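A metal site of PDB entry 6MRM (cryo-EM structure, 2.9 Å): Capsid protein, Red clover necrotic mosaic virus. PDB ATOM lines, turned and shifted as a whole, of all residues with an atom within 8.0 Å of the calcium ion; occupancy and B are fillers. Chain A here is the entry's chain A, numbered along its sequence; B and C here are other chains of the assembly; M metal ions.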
ATOM      1  N   ASP A 125      -1.109  13.308  -4.095  1.00  0.00           N
ATOM      2  CA  ASP A 125      -0.748  14.364  -5.040  1.00  0.00           C
ATOM      3  C   ASP A 125      -0.309  15.617  -4.319  1.00  0.00           C
ATOM      4  O   ASP A 125      -0.771  15.920  -3.222  1.00  0.00           O
ATOM      5  CB  ASP A 125      -1.900  14.712  -5.955  1.00  0.00           C
ATOM      6  CG  ASP A 125      -1.776  14.090  -7.297  1.00  0.00           C
ATOM      7  OD1 ASP A 125      -0.628  14.009  -7.779  1.00  0.00           O
ATOM      8  OD2 ASP A 125      -2.790  13.697  -7.903  1.00  0.00           O
ATOM      9  N   PRO A 126       0.585  16.376  -4.905  1.00  0.00           N
ATOM     10  CA  PRO A 126       0.826  17.733  -4.435  1.00  0.00           C
ATOM     11  C   PRO A 126      -0.168  18.703  -5.067  1.00  0.00           C
ATOM     12  O   PRO A 126      -0.453  19.757  -4.498  1.00  0.00           O
ATOM     13  CB  PRO A 126       2.258  18.009  -4.860  1.00  0.00           C
ATOM     14  CG  PRO A 126       2.463  17.159  -6.035  1.00  0.00           C
ATOM     15  CD  PRO A 126       1.657  15.921  -5.812  1.00  0.00           C
ATOM     16  N   ASP A 127      -0.682  18.355  -6.244  1.00  0.00           N
ATOM     17  CA  ASP A 127      -1.838  19.056  -6.772  1.00  0.00           C
ATOM     18  C   ASP A 127      -3.075  18.718  -5.969  1.00  0.00           C
ATOM     19  O   ASP A 127      -3.116  17.738  -5.222  1.00  0.00           O
ATOM     20  CB  ASP A 127      -2.104  18.679  -8.226  1.00  0.00           C
ATOM     21  CG  ASP A 127      -1.362  19.534  -9.200  1.00  0.00           C
ATOM     22  OD1 ASP A 127      -1.192  20.721  -8.887  1.00  0.00           O
ATOM     23  OD2 ASP A 127      -0.975  19.043 -10.270  1.00  0.00           O
ATOM     24  N   SER A 128      -4.100  19.523  -6.152  1.00  0.00           N
ATOM     25  CA  SER A 128      -5.428  19.178  -5.669  1.00  0.00           C
ATOM     26  C   SER A 128      -6.440  19.206  -6.796  1.00  0.00           C
ATOM     27  O   SER A 128      -7.649  19.149  -6.528  1.00  0.00           O
ATOM     28  CB  SER A 128      -5.851  20.104  -4.537  1.00  0.00           C
ATOM     29  OG  SER A 128      -5.994  21.429  -5.006  1.00  0.00           O
ATOM     30  N   GLN A 129      -5.983  19.289  -8.044  1.00  0.00           N
ATOM     31  CA  GLN A 129      -6.864  19.329  -9.186  1.00  0.00           C
ATOM     32  C   GLN A 129      -6.459  18.361 -10.281  1.00  0.00           C
ATOM     33  O   GLN A 129      -6.997  18.444 -11.389  1.00  0.00           O
ATOM     34  CB  GLN A 129      -6.942  20.737  -9.766  1.00  0.00           C
ATOM     35  CG  GLN A 129      -7.626  21.729  -8.888  1.00  0.00           C
ATOM     36  CD  GLN A 129      -7.593  23.108  -9.461  1.00  0.00           C
ATOM     37  OE1 GLN A 129      -6.977  23.347 -10.493  1.00  0.00           O
ATOM     38  NE2 GLN A 129      -8.266  24.040  -8.802  1.00  0.00           N
ATOM     39  N   ASP A 130      -5.501  17.473 -10.030  1.00  0.00           N
ATOM     40  CA  ASP A 130      -5.211  16.424 -10.996  1.00  0.00           C
ATOM     41  C   ASP A 130      -6.370  15.441 -11.057  1.00  0.00           C
ATOM     42  O   ASP A 130      -7.168  15.317 -10.128  1.00  0.00           O
ATOM     43  CB  ASP A 130      -3.931  15.676 -10.639  1.00  0.00           C
ATOM     44  CG  ASP A 130      -2.688  16.485 -10.928  1.00  0.00           C
ATOM     45  OD1 ASP A 130      -2.747  17.383 -11.782  1.00  0.00           O
ATOM     46  OD2 ASP A 130      -1.643  16.193 -10.312  1.00  0.00           O
ATOM     47  N   SER A 131      -6.458  14.734 -12.173  1.00  0.00           N
ATOM     48  CA  SER A 131      -7.539  13.780 -12.374  1.00  0.00           C
ATOM     49  C   SER A 131      -7.209  12.472 -11.662  1.00  0.00           C
ATOM     50  O   SER A 131      -6.180  12.336 -11.002  1.00  0.00           O
ATOM     51  CB  SER A 131      -7.778  13.571 -13.859  1.00  0.00           C
ATOM     52  OG  SER A 131      -6.666  12.955 -14.463  1.00  0.00           O
ATOM     53  N   TYR A 142       3.173   8.243  -8.355  1.00  0.00           N
ATOM     54  CA  TYR A 142       3.012   9.465  -7.604  1.00  0.00           C
ATOM     55  C   TYR A 142       4.219   9.701  -6.711  1.00  0.00           C
ATOM     56  O   TYR A 142       5.130   8.876  -6.627  1.00  0.00           O
ATOM     57  CB  TYR A 142       1.721   9.420  -6.800  1.00  0.00           C
ATOM     58  CG  TYR A 142       0.493   9.594  -7.645  1.00  0.00           C
ATOM     59  CD1 TYR A 142       0.017  10.854  -7.930  1.00  0.00           C
ATOM     60  CD2 TYR A 142      -0.175   8.515  -8.183  1.00  0.00           C
ATOM     61  CE1 TYR A 142      -1.103  11.033  -8.704  1.00  0.00           C
ATOM     62  CE2 TYR A 142      -1.303   8.685  -8.949  1.00  0.00           C
ATOM     63  CZ  TYR A 142      -1.758   9.950  -9.207  1.00  0.00           C
ATOM     64  OH  TYR A 142      -2.878  10.129  -9.981  1.00  0.00           O
ATOM     65  N   LYS A 176      -6.119  24.503  -6.241  1.00  0.00           N
ATOM     66  CA  LYS A 176      -4.737  24.136  -6.488  1.00  0.00           C
ATOM     67  C   LYS A 176      -3.751  24.937  -5.663  1.00  0.00           C
ATOM     68  O   LYS A 176      -2.654  24.442  -5.374  1.00  0.00           O
ATOM     69  CB  LYS A 176      -4.500  24.326  -7.978  1.00  0.00           C
ATOM     70  CG  LYS A 176      -3.256  23.766  -8.569  1.00  0.00           C
ATOM     71  CD  LYS A 176      -3.379  23.908 -10.065  1.00  0.00           C
ATOM     72  CE  LYS A 176      -2.223  23.290 -10.784  1.00  0.00           C
ATOM     73  NZ  LYS A 176      -2.398  23.403 -12.248  1.00  0.00           N
ATOM     74  N   ALA B  93       8.395  17.933 -18.374  1.00  0.00           N
ATOM     75  CA  ALA B  93       7.421  18.597 -17.524  1.00  0.00           C
ATOM     76  C   ALA B  93       6.166  17.770 -17.333  1.00  0.00           C
ATOM     77  O   ALA B  93       5.398  18.055 -16.415  1.00  0.00           O
ATOM     78  CB  ALA B  93       7.047  19.944 -18.114  1.00  0.00           C
ATOM     79  N   ALA B  94       5.948  16.758 -18.162  1.00  0.00           N
ATOM     80  CA  ALA B  94       4.781  15.917 -17.954  1.00  0.00           C
ATOM     81  C   ALA B  94       4.926  15.010 -16.752  1.00  0.00           C
ATOM     82  O   ALA B  94       3.926  14.472 -16.274  1.00  0.00           O
ATOM     83  CB  ALA B  94       4.510  15.084 -19.206  1.00  0.00           C
ATOM     84  N   ASN B  95       6.134  14.826 -16.252  1.00  0.00           N
ATOM     85  CA  ASN B  95       6.365  13.927 -15.126  1.00  0.00           C
ATOM     86  C   ASN B  95       6.219  14.594 -13.776  1.00  0.00           C
ATOM     87  O   ASN B  95       6.234  13.903 -12.765  1.00  0.00           O
ATOM     88  CB  ASN B  95       7.749  13.311 -15.201  1.00  0.00           C
ATOM     89  CG  ASN B  95       7.885  12.340 -16.314  1.00  0.00           C
ATOM     90  OD1 ASN B  95       6.970  11.598 -16.605  1.00  0.00           O
ATOM     91  ND2 ASN B  95       9.055  12.302 -16.933  1.00  0.00           N
ATOM     92  N   TYR B  96       6.111  15.916 -13.716  1.00  0.00           N
ATOM     93  CA  TYR B  96       6.262  16.616 -12.455  1.00  0.00           C
ATOM     94  C   TYR B  96       5.115  17.583 -12.270  1.00  0.00           C
ATOM     95  O   TYR B  96       4.320  17.832 -13.179  1.00  0.00           O
ATOM     96  CB  TYR B  96       7.588  17.342 -12.410  1.00  0.00           C
ATOM     97  CG  TYR B  96       8.781  16.429 -12.470  1.00  0.00           C
ATOM     98  CD1 TYR B  96       9.245  15.794 -11.333  1.00  0.00           C
ATOM     99  CD2 TYR B  96       9.432  16.211 -13.657  1.00  0.00           C
ATOM    100  CE1 TYR B  96      10.332  14.971 -11.387  1.00  0.00           C
ATOM    101  CE2 TYR B  96      10.521  15.381 -13.719  1.00  0.00           C
ATOM    102  CZ  TYR B  96      10.960  14.762 -12.587  1.00  0.00           C
ATOM    103  OH  TYR B  96      12.048  13.931 -12.649  1.00  0.00           O
ATOM    104  N   ASP B  97       5.027  18.149 -11.065  1.00  0.00           N
ATOM    105  CA  ASP B  97       3.998  19.131 -10.760  1.00  0.00           C
ATOM    106  C   ASP B  97       4.519  20.428 -10.193  1.00  0.00           C
ATOM    107  O   ASP B  97       3.733  21.357 -10.031  1.00  0.00           O
ATOM    108  CB  ASP B  97       2.972  18.539  -9.784  1.00  0.00           C
ATOM    109  CG  ASP B  97       1.892  17.772 -10.489  1.00  0.00           C
ATOM    110  OD1 ASP B  97       1.518  18.182 -11.603  1.00  0.00           O
ATOM    111  OD2 ASP B  97       1.400  16.765  -9.940  1.00  0.00           O
ATOM    112  N   MET B  98       5.805  20.536  -9.878  1.00  0.00           N
ATOM    113  CA  MET B  98       6.369  21.771  -9.371  1.00  0.00           C
ATOM    114  C   MET B  98       7.615  22.075 -10.167  1.00  0.00           C
ATOM    115  O   MET B  98       8.366  21.161 -10.505  1.00  0.00           O
ATOM    116  CB  MET B  98       6.721  21.659  -7.890  1.00  0.00           C
ATOM    117  CG  MET B  98       5.622  21.173  -6.988  1.00  0.00           C
ATOM    118  SD  MET B  98       4.204  22.247  -6.900  1.00  0.00           S
ATOM    119  CE  MET B  98       4.827  23.544  -5.866  1.00  0.00           C
ATOM    120  N   PHE B 166       3.303  25.675  -9.775  1.00  0.00           N
ATOM    121  CA  PHE B 166       2.683  24.485 -10.322  1.00  0.00           C
ATOM    122  C   PHE B 166       2.859  24.389 -11.828  1.00  0.00           C
ATOM    123  O   PHE B 166       2.856  25.387 -12.544  1.00  0.00           O
ATOM    124  CB  PHE B 166       1.202  24.460  -9.981  1.00  0.00           C
ATOM    125  CG  PHE B 166       0.932  24.175  -8.559  1.00  0.00           C
ATOM    126  CD1 PHE B 166       0.942  22.881  -8.103  1.00  0.00           C
ATOM    127  CD2 PHE B 166       0.690  25.186  -7.659  1.00  0.00           C
ATOM    128  CE1 PHE B 166       0.688  22.594  -6.788  1.00  0.00           C
ATOM    129  CE2 PHE B 166       0.444  24.907  -6.338  1.00  0.00           C
ATOM    130  CZ  PHE B 166       0.444  23.604  -5.902  1.00  0.00           C
ATOM    131  N   VAL B 167       3.019  23.163 -12.296  1.00  0.00           N
ATOM    132  CA  VAL B 167       3.079  22.891 -13.721  1.00  0.00           C
ATOM    133  C   VAL B 167       1.656  22.743 -14.233  1.00  0.00           C
ATOM    134  O   VAL B 167       0.866  21.974 -13.674  1.00  0.00           O
ATOM    135  CB  VAL B 167       3.910  21.639 -13.998  1.00  0.00           C
ATOM    136  CG1 VAL B 167       3.926  21.327 -15.463  1.00  0.00           C
ATOM    137  CG2 VAL B 167       5.310  21.833 -13.492  1.00  0.00           C
ATOM    138  N   ALA B 168       1.327  23.477 -15.288  1.00  0.00           N
ATOM    139  CA  ALA B 168      -0.067  23.598 -15.719  1.00  0.00           C
ATOM    140  C   ALA B 168      -0.520  22.327 -16.424  1.00  0.00           C
ATOM    141  O   ALA B 168      -0.214  22.124 -17.604  1.00  0.00           O
ATOM    142  CB  ALA B 168      -0.217  24.801 -16.633  1.00  0.00           C
ATOM    143  N   ASP B 169      -1.283  21.484 -15.732  1.00  0.00           N
ATOM    144  CA  ASP B 169      -1.991  20.373 -16.373  1.00  0.00           C
ATOM    145  C   ASP B 169      -3.469  20.569 -16.048  1.00  0.00           C
ATOM    146  O   ASP B 169      -4.046  19.787 -15.283  1.00  0.00           O
ATOM    147  CB  ASP B 169      -1.489  19.031 -15.863  1.00  0.00           C
ATOM    148  CG  ASP B 169      -0.041  18.791 -16.179  1.00  0.00           C
ATOM    149  OD1 ASP B 169       0.434  19.301 -17.204  1.00  0.00           O
ATOM    150  OD2 ASP B 169       0.625  18.086 -15.386  1.00  0.00           O
ATOM    151  N   ASN B 170      -4.088  21.518 -16.732  1.00  0.00           N
ATOM    152  CA  ASN B 170      -5.336  22.130 -16.333  1.00  0.00           C
ATOM    153  C   ASN B 170      -5.487  23.159 -17.458  1.00  0.00           C
ATOM    154  O   ASN B 170      -4.540  23.262 -18.241  1.00  0.00           O
ATOM    155  CB  ASN B 170      -5.105  22.710 -14.942  1.00  0.00           C
ATOM    156  CG  ASN B 170      -6.247  22.402 -13.982  1.00  0.00           C
ATOM    157  OD1 ASN B 170      -7.235  21.802 -14.369  1.00  0.00           O
ATOM    158  ND2 ASN B 170      -6.079  22.793 -12.727  1.00  0.00           N
ATOM    159  N   GLY B 209       8.272  17.441  -6.743  1.00  0.00           N
ATOM    160  CA  GLY B 209       7.626  16.129  -6.741  1.00  0.00           C
ATOM    161  C   GLY B 209       6.960  15.589  -7.985  1.00  0.00           C
ATOM    162  O   GLY B 209       6.220  16.282  -8.681  1.00  0.00           O
ATOM    163  N   PRO B 210       7.206  14.319  -8.267  1.00  0.00           N
ATOM    164  CA  PRO B 210       6.774  13.744  -9.546  1.00  0.00           C
ATOM    165  C   PRO B 210       5.299  13.419  -9.642  1.00  0.00           C
ATOM    166  O   PRO B 210       4.523  13.730  -8.738  1.00  0.00           O
ATOM    167  CB  PRO B 210       7.621  12.473  -9.646  1.00  0.00           C
ATOM    168  CG  PRO B 210       7.888  12.100  -8.278  1.00  0.00           C
ATOM    169  CD  PRO B 210       8.036  13.372  -7.504  1.00  0.00           C
ATOM    170  N   GLN B 211       4.919  12.768 -10.739  1.00  0.00           N
ATOM    171  CA  GLN B 211       3.541  12.667 -11.176  1.00  0.00           C
ATOM    172  C   GLN B 211       3.481  11.587 -12.234  1.00  0.00           C
ATOM    173  O   GLN B 211       4.473  11.373 -12.939  1.00  0.00           O
ATOM    174  CB  GLN B 211       3.068  13.996 -11.766  1.00  0.00           C
ATOM    175  CG  GLN B 211       1.578  14.149 -11.979  1.00  0.00           C
ATOM    176  CD  GLN B 211       1.248  15.348 -12.796  1.00  0.00           C
ATOM    177  OE1 GLN B 211       2.115  15.970 -13.394  1.00  0.00           O
ATOM    178  NE2 GLN B 211      -0.030  15.729 -12.811  1.00  0.00           N
ATOM    179  N   PRO B 212       2.363  10.871 -12.364  1.00  0.00           N
ATOM    180  CA  PRO B 212       2.152  10.097 -13.577  1.00  0.00           C
ATOM    181  C   PRO B 212       2.020  11.037 -14.767  1.00  0.00           C
ATOM    182  O   PRO B 212       1.533  12.159 -14.639  1.00  0.00           O
ATOM    183  CB  PRO B 212       0.850   9.353 -13.305  1.00  0.00           C
ATOM    184  CG  PRO B 212       0.199  10.104 -12.243  1.00  0.00           C
ATOM    185  CD  PRO B 212       1.301  10.620 -11.388  1.00  0.00           C
ATOM    186  N   ALA B 214       1.503  13.338 -17.770  1.00  0.00           N
ATOM    187  CA  ALA B 214       0.428  14.003 -18.487  1.00  0.00           C
ATOM    188  C   ALA B 214       0.490  13.593 -19.948  1.00  0.00           C
ATOM    189  O   ALA B 214       1.570  13.510 -20.525  1.00  0.00           O
ATOM    190  CB  ALA B 214       0.546  15.514 -18.344  1.00  0.00           C
ATOM    191  N   LYS C 331      -4.052   9.597 -23.500  1.00  0.00           N
ATOM    192  CA  LYS C 331      -4.788   9.515 -22.248  1.00  0.00           C
ATOM    193  C   LYS C 331      -6.272   9.328 -22.579  1.00  0.00           C
ATOM    194  O   LYS C 331      -6.653   9.035 -23.714  1.00  0.00           O
ATOM    195  CB  LYS C 331      -4.537  10.733 -21.374  1.00  0.00           C
ATOM    196  CG  LYS C 331      -3.151  10.762 -20.781  1.00  0.00           C
ATOM    197  CD  LYS C 331      -2.959  12.001 -19.938  1.00  0.00           C
ATOM    198  CE  LYS C 331      -3.756  11.918 -18.669  1.00  0.00           C
ATOM    199  NZ  LYS C 331      -3.482  13.054 -17.767  1.00  0.00           N
HETATM  200 CA    CA M   1      -0.461  17.686 -12.034  1.00  0.00          CA
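The calcium ion is bound by OD1 of Asp 97 of chain B (2.1 Å), NE2 of Gln 211 of chain B (2.1 Å), OD2 of Asp 127 (2.3 Å), OD1 of Asp 130 (2.3 Å) and OD2 of Asp 130 (2.6 Å).
The calcium ion has five donor atoms within binding distance.
Slightly farther from the calcium ion lies OD2 of Asp 97 of chain B (2.9 Å).
O of Asp 97 of chain B is in hydrogen-bond range of N of Val 167 of chain B (3.0 Å).
The backbone NH of Asp 97 of chain B lies within hydrogen-bond range of the backbone carbonyl oxygen of Gly 209 of chain B.
OE1 of Gln 211 of chain B sits close to OD2 of Asp 169 of chain B, at 3.3 Å.
The backbone carbonyl oxygen (O) of Tyr 96 of chain B sits close to the side-chain amide oxygen (OE1) of Gln 211 of chain B (2.9 Å).
N of Gln 211 of chain B sits at hydrogen-bond distance from O of Asn 95 of chain B, 2.7 Å away.
OD2 of Asp 169 of chain B touches the calcium ion, at 3.5 Å.
Within 4 Å of the calcium ion: Asp 127, Asp 130, Asp 97 of chain B, Asp 169 of chain B and Gln 211 of chain B.
The nearest printed residue that does not touch the calcium ion is Val 167 of chain B (4.8 Å).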
